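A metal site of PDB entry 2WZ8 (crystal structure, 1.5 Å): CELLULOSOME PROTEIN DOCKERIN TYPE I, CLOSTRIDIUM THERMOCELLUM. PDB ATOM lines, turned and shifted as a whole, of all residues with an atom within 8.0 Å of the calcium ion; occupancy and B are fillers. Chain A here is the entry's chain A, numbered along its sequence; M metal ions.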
ATOM      1  N   TYR A  11     -32.273   0.503  24.631  1.00  0.00           N
ATOM      2  CA  TYR A  11     -30.855   0.330  24.930  1.00  0.00           C
ATOM      3  C   TYR A  11     -30.020   1.341  24.148  1.00  0.00           C
ATOM      4  O   TYR A  11     -30.007   1.355  22.905  1.00  0.00           O
ATOM      5  CB  TYR A  11     -30.373  -1.083  24.594  1.00  0.00           C
ATOM      6  CG  TYR A  11     -31.228  -2.157  25.222  1.00  0.00           C
ATOM      7  CD1 TYR A  11     -30.936  -2.651  26.485  1.00  0.00           C
ATOM      8  CD2 TYR A  11     -32.378  -2.624  24.595  1.00  0.00           C
ATOM      9  CE1 TYR A  11     -31.736  -3.624  27.083  1.00  0.00           C
ATOM     10  CE2 TYR A  11     -33.194  -3.595  25.206  1.00  0.00           C
ATOM     11  CZ  TYR A  11     -32.843  -4.101  26.431  1.00  0.00           C
ATOM     12  OH  TYR A  11     -33.665  -5.053  27.031  1.00  0.00           O
ATOM     13  N   GLU A  12     -29.301   2.157  24.890  1.00  0.00           N
ATOM     14  CA  GLU A  12     -28.375   3.117  24.273  1.00  0.00           C
ATOM     15  C   GLU A  12     -27.188   2.371  23.714  1.00  0.00           C
ATOM     16  O   GLU A  12     -26.663   1.451  24.337  1.00  0.00           O
ATOM     17  CB  GLU A  12     -27.913   4.156  25.283  1.00  0.00           C
ATOM     18  CG  GLU A  12     -29.017   5.074  25.739  1.00  0.00           C
ATOM     19  CD  GLU A  12     -29.537   6.091  24.698  1.00  0.00           C
ATOM     20  OE1 GLU A  12     -28.925   6.232  23.603  1.00  0.00           O
ATOM     21  OE2 GLU A  12     -30.570   6.752  25.015  1.00  0.00           O
ATOM     22  N   ALA A  13     -26.719   2.793  22.544  1.00  0.00           N
ATOM     23  CA  ALA A  13     -25.545   2.154  21.953  1.00  0.00           C
ATOM     24  C   ALA A  13     -24.315   2.263  22.890  1.00  0.00           C
ATOM     25  O   ALA A  13     -23.494   1.355  23.019  1.00  0.00           O
ATOM     26  CB  ALA A  13     -25.244   2.801  20.606  1.00  0.00           C
ATOM     27  N   GLU A  14     -24.209   3.416  23.549  1.00  0.00           N
ATOM     28  CA  GLU A  14     -23.096   3.746  24.452  1.00  0.00           C
ATOM     29  C   GLU A  14     -23.226   3.157  25.852  1.00  0.00           C
ATOM     30  O   GLU A  14     -22.375   3.380  26.694  1.00  0.00           O
ATOM     31  CB  GLU A  14     -22.948   5.258  24.584  1.00  0.00           C
ATOM     32  CG  GLU A  14     -24.157   5.966  25.247  1.00  0.00           C
ATOM     33  CD  GLU A  14     -25.273   6.408  24.293  1.00  0.00           C
ATOM     34  OE1 GLU A  14     -25.385   5.859  23.151  1.00  0.00           O
ATOM     35  OE2 GLU A  14     -26.047   7.307  24.661  1.00  0.00           O
ATOM     36  N   ASP A  15     -24.312   2.439  26.098  1.00  0.00           N
ATOM     37  CA  ASP A  15     -24.522   1.800  27.410  1.00  0.00           C
ATOM     38  C   ASP A  15     -23.242   1.088  27.822  1.00  0.00           C
ATOM     39  O   ASP A  15     -22.665   0.338  27.036  1.00  0.00           O
ATOM     40  CB  ASP A  15     -25.676   0.799  27.307  1.00  0.00           C
ATOM     41  CG  ASP A  15     -26.092   0.185  28.635  1.00  0.00           C
ATOM     42  OD1 ASP A  15     -25.270  -0.056  29.502  1.00  0.00           O
ATOM     43  OD2 ASP A  15     -27.278  -0.133  28.741  1.00  0.00           O
ATOM     44  N   GLN A  27     -18.851   8.201  21.288  1.00  0.00           N
ATOM     45  CA  GLN A  27     -18.554   9.618  21.049  1.00  0.00           C
ATOM     46  C   GLN A  27     -19.755  10.466  21.432  1.00  0.00           C
ATOM     47  O   GLN A  27     -20.903  10.025  21.385  1.00  0.00           O
ATOM     48  CB  GLN A  27     -18.087   9.862  19.607  1.00  0.00           C
ATOM     49  CG  GLN A  27     -16.671   9.359  19.378  1.00  0.00           C
ATOM     50  CD  GLN A  27     -16.093   9.600  18.007  1.00  0.00           C
ATOM     51  OE1 GLN A  27     -16.783   9.930  17.016  1.00  0.00           O
ATOM     52  NE2 GLN A  27     -14.791   9.362  17.911  1.00  0.00           N
ATOM     53  N   ASP A  29     -22.436  13.540  21.230  1.00  0.00           N
ATOM     54  CA  ASP A  29     -23.228  14.360  20.303  1.00  0.00           C
ATOM     55  C   ASP A  29     -24.455  14.812  21.034  1.00  0.00           C
ATOM     56  O   ASP A  29     -25.264  13.984  21.425  1.00  0.00           O
ATOM     57  CB  ASP A  29     -23.637  13.554  19.083  1.00  0.00           C
ATOM     58  CG  ASP A  29     -24.311  14.377  17.998  1.00  0.00           C
ATOM     59  OD1 ASP A  29     -24.599  15.569  18.241  1.00  0.00           O
ATOM     60  OD2 ASP A  29     -24.493  13.850  16.879  1.00  0.00           O
ATOM     61  N   ALA A  31     -26.983  16.068  19.964  1.00  0.00           N
ATOM     62  CA  ALA A  31     -28.165  15.785  19.144  1.00  0.00           C
ATOM     63  C   ALA A  31     -28.633  14.335  19.292  1.00  0.00           C
ATOM     64  O   ALA A  31     -29.755  14.017  18.926  1.00  0.00           O
ATOM     65  CB  ALA A  31     -27.896  16.033  17.668  1.00  0.00           C
ATOM     66  N   ALA A  32     -27.800  13.478  19.882  1.00  0.00           N
ATOM     67  CA  ALA A  32     -28.108  12.047  20.079  1.00  0.00           C
ATOM     68  C   ALA A  32     -28.809  11.766  21.388  1.00  0.00           C
ATOM     69  O   ALA A  32     -28.626  12.473  22.385  1.00  0.00           O
ATOM     70  CB  ALA A  32     -26.794  11.210  19.986  1.00  0.00           C
ATOM     71  N   SER A  33     -29.612  10.713  21.399  1.00  0.00           N
ATOM     72  CA  SER A  33     -30.191  10.211  22.639  1.00  0.00           C
ATOM     73  C   SER A  33     -29.121   9.903  23.658  1.00  0.00           C
ATOM     74  O   SER A  33     -28.121   9.223  23.367  1.00  0.00           O
ATOM     75  CB  SER A  33     -31.071   9.004  22.365  1.00  0.00           C
ATOM     76  OG  SER A  33     -31.743   8.542  23.504  1.00  0.00           O
ATOM     77  N   GLY A  34     -29.285  10.463  24.844  1.00  0.00           N
ATOM     78  CA  GLY A  34     -28.321  10.253  25.909  1.00  0.00           C
ATOM     79  C   GLY A  34     -27.041  11.055  25.772  1.00  0.00           C
ATOM     80  O   GLY A  34     -26.123  10.956  26.605  1.00  0.00           O
ATOM     81  N   GLY A  35     -26.985  11.834  24.708  1.00  0.00           N
ATOM     82  CA  GLY A  35     -25.830  12.662  24.385  1.00  0.00           C
ATOM     83  C   GLY A  35     -24.616  11.945  23.839  1.00  0.00           C
ATOM     84  O   GLY A  35     -23.543  12.524  23.680  1.00  0.00           O
ATOM     85  N   GLN A  36     -24.808  10.701  23.453  1.00  0.00           N
ATOM     86  CA  GLN A  36     -23.722   9.918  22.859  1.00  0.00           C
ATOM     87  C   GLN A  36     -24.259   8.948  21.810  1.00  0.00           C
ATOM     88  O   GLN A  36     -25.455   8.594  21.800  1.00  0.00           O
ATOM     89  CB  GLN A  36     -22.986   9.074  23.926  1.00  0.00           C
ATOM     90  CG  GLN A  36     -22.237   9.827  25.013  1.00  0.00           C
ATOM     91  CD  GLN A  36     -21.555   8.812  25.950  1.00  0.00           C
ATOM     92  OE1 GLN A  36     -20.528   8.275  25.606  1.00  0.00           O
ATOM     93  NE2 GLN A  36     -22.140   8.543  27.082  1.00  0.00           N
ATOM     94  N   TYR A  37     -23.325   8.459  21.016  1.00  0.00           N
ATOM     95  CA  TYR A  37     -23.563   7.414  19.977  1.00  0.00           C
ATOM     96  C   TYR A  37     -22.310   6.578  19.859  1.00  0.00           C
ATOM     97  O   TYR A  37     -21.279   6.864  20.498  1.00  0.00           O
ATOM     98  CB  TYR A  37     -23.966   8.015  18.643  1.00  0.00           C
ATOM     99  CG  TYR A  37     -22.832   8.759  17.996  1.00  0.00           C
ATOM    100  CD1 TYR A  37     -22.007   8.132  17.079  1.00  0.00           C
ATOM    101  CD2 TYR A  37     -22.566  10.076  18.349  1.00  0.00           C
ATOM    102  CE1 TYR A  37     -20.922   8.778  16.547  1.00  0.00           C
ATOM    103  CE2 TYR A  37     -21.471  10.742  17.779  1.00  0.00           C
ATOM    104  CZ  TYR A  37     -20.678  10.096  16.888  1.00  0.00           C
ATOM    105  OH  TYR A  37     -19.583  10.726  16.323  1.00  0.00           O
ATOM    106  N   VAL A  38     -22.395   5.507  19.070  1.00  0.00           N
ATOM    107  CA  VAL A  38     -21.222   4.692  18.758  1.00  0.00           C
ATOM    108  C   VAL A  38     -20.922   4.816  17.276  1.00  0.00           C
ATOM    109  O   VAL A  38     -21.770   4.656  16.445  1.00  0.00           O
ATOM    110  CB  VAL A  38     -21.392   3.218  19.205  1.00  0.00           C
ATOM    111  CG1 VAL A  38     -20.230   2.374  18.727  1.00  0.00           C
ATOM    112  CG2 VAL A  38     -21.466   3.166  20.694  1.00  0.00           C
ATOM    113  N   GLN A  67     -32.078   3.584  15.899  1.00  0.00           N
ATOM    114  CA  GLN A  67     -31.872   5.030  15.689  1.00  0.00           C
ATOM    115  C   GLN A  67     -30.418   5.255  15.323  1.00  0.00           C
ATOM    116  O   GLN A  67     -29.529   4.829  16.017  1.00  0.00           O
ATOM    117  CB  GLN A  67     -32.271   5.849  16.912  1.00  0.00           C
ATOM    118  CG  GLN A  67     -32.181   7.358  16.661  1.00  0.00           C
ATOM    119  CD  GLN A  67     -32.990   8.184  17.613  1.00  0.00           C
ATOM    120  OE1 GLN A  67     -32.436   8.983  18.410  1.00  0.00           O
ATOM    121  NE2 GLN A  67     -34.287   8.014  17.561  1.00  0.00           N
ATOM    122  N   TYR A 111     -30.442  12.118  13.333  1.00  0.00           N
ATOM    123  CA  TYR A 111     -30.758  10.746  13.729  1.00  0.00           C
ATOM    124  C   TYR A 111     -32.193  10.387  13.372  1.00  0.00           C
ATOM    125  O   TYR A 111     -33.123  11.107  13.723  1.00  0.00           O
ATOM    126  CB  TYR A 111     -30.532  10.535  15.243  1.00  0.00           C
ATOM    127  CG  TYR A 111     -29.090  10.737  15.618  1.00  0.00           C
ATOM    128  CD1 TYR A 111     -28.177   9.686  15.583  1.00  0.00           C
ATOM    129  CD2 TYR A 111     -28.626  11.969  16.035  1.00  0.00           C
ATOM    130  CE1 TYR A 111     -26.853   9.862  15.916  1.00  0.00           C
ATOM    131  CE2 TYR A 111     -27.288  12.156  16.351  1.00  0.00           C
ATOM    132  CZ  TYR A 111     -26.403  11.095  16.315  1.00  0.00           C
ATOM    133  OH  TYR A 111     -25.062  11.291  16.634  1.00  0.00           O
ATOM    134  N   ILE A 141     -24.627   4.404  15.323  1.00  0.00           N
ATOM    135  CA  ILE A 141     -25.787   3.891  16.057  1.00  0.00           C
ATOM    136  C   ILE A 141     -25.956   4.664  17.360  1.00  0.00           C
ATOM    137  O   ILE A 141     -25.022   4.769  18.147  1.00  0.00           O
ATOM    138  CB  ILE A 141     -25.712   2.388  16.317  1.00  0.00           C
ATOM    139  CG1 ILE A 141     -25.442   1.632  15.007  1.00  0.00           C
ATOM    140  CG2 ILE A 141     -26.965   1.877  17.064  1.00  0.00           C
ATOM    141  CD1 ILE A 141     -26.516   1.610  14.054  1.00  0.00           C
ATOM    142  N   ASP A 142     -27.141   5.226  17.527  1.00  0.00           N
ATOM    143  CA  ASP A 142     -27.499   6.013  18.726  1.00  0.00           C
ATOM    144  C   ASP A 142     -28.063   5.131  19.858  1.00  0.00           C
ATOM    145  O   ASP A 142     -27.636   5.173  21.022  1.00  0.00           O
ATOM    146  CB  ASP A 142     -28.474   7.113  18.302  1.00  0.00           C
ATOM    147  CG  ASP A 142     -28.861   8.052  19.426  1.00  0.00           C
ATOM    148  OD1 ASP A 142     -28.274   7.976  20.534  1.00  0.00           O
ATOM    149  OD2 ASP A 142     -29.705   8.942  19.148  1.00  0.00           O
ATOM    150  N   LYS A 143     -29.075   4.365  19.494  1.00  0.00           N
ATOM    151  CA  LYS A 143     -29.802   3.471  20.402  1.00  0.00           C
ATOM    152  C   LYS A 143     -30.640   2.501  19.590  1.00  0.00           C
ATOM    153  O   LYS A 143     -30.816   2.671  18.393  1.00  0.00           O
ATOM    154  CB  LYS A 143     -30.699   4.257  21.379  1.00  0.00           C
ATOM    155  CG  LYS A 143     -31.735   5.086  20.723  1.00  0.00           C
ATOM    156  CD  LYS A 143     -32.769   5.603  21.722  1.00  0.00           C
ATOM    157  CE  LYS A 143     -33.729   6.594  21.131  1.00  0.00           C
ATOM    158  NZ  LYS A 143     -34.837   7.021  22.055  1.00  0.00           N
ATOM    159  N   ILE A 144     -31.135   1.474  20.264  1.00  0.00           N
ATOM    160  CA  ILE A 144     -32.160   0.572  19.749  1.00  0.00           C
ATOM    161  C   ILE A 144     -33.308   0.448  20.732  1.00  0.00           C
ATOM    162  O   ILE A 144     -33.163   0.712  21.930  1.00  0.00           O
ATOM    163  CB  ILE A 144     -31.570  -0.825  19.399  1.00  0.00           C
ATOM    164  CG1 ILE A 144     -31.194  -1.621  20.639  1.00  0.00           C
ATOM    165  CG2 ILE A 144     -30.393  -0.746  18.380  1.00  0.00           C
ATOM    166  CD1 ILE A 144     -30.753  -3.032  20.349  1.00  0.00           C
HETATM  167 CA    CA M   1     -27.263   7.277  22.425  1.00  0.00          CA
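The backbone carbonyl oxygen of Asp 142 lies close to the backbone NH of Ala 13 (3.0 Å). The side-chain carboxylate (OD2) of Asp 142 sits close to the side-chain amide oxygen (OE1) of Gln 67 (2.8 Å).
Of the 21 residues printed, 5 come within 4 Å of the calcium ion. The nearest printed residue that does not touch the calcium ion is Tyr 37 (4.3 Å).
The side-chain carboxylate (OD1) of Asp 142 is bound to the calcium ion (2.3 Å). OE1 of Glu 12 binds the calcium ion (2.3 Å). The calcium ion is bound by the backbone carbonyl oxygen (O) of Gln 36, 2.3 Å away. O of Ser 33 is bound to the calcium ion, at 2.3 Å. The calcium ion is bound by OE1 of Glu 14 (2.5 Å). The calcium ion is bound by OE2 of Glu 14. The calcium ion is bound by O of Asp 142.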
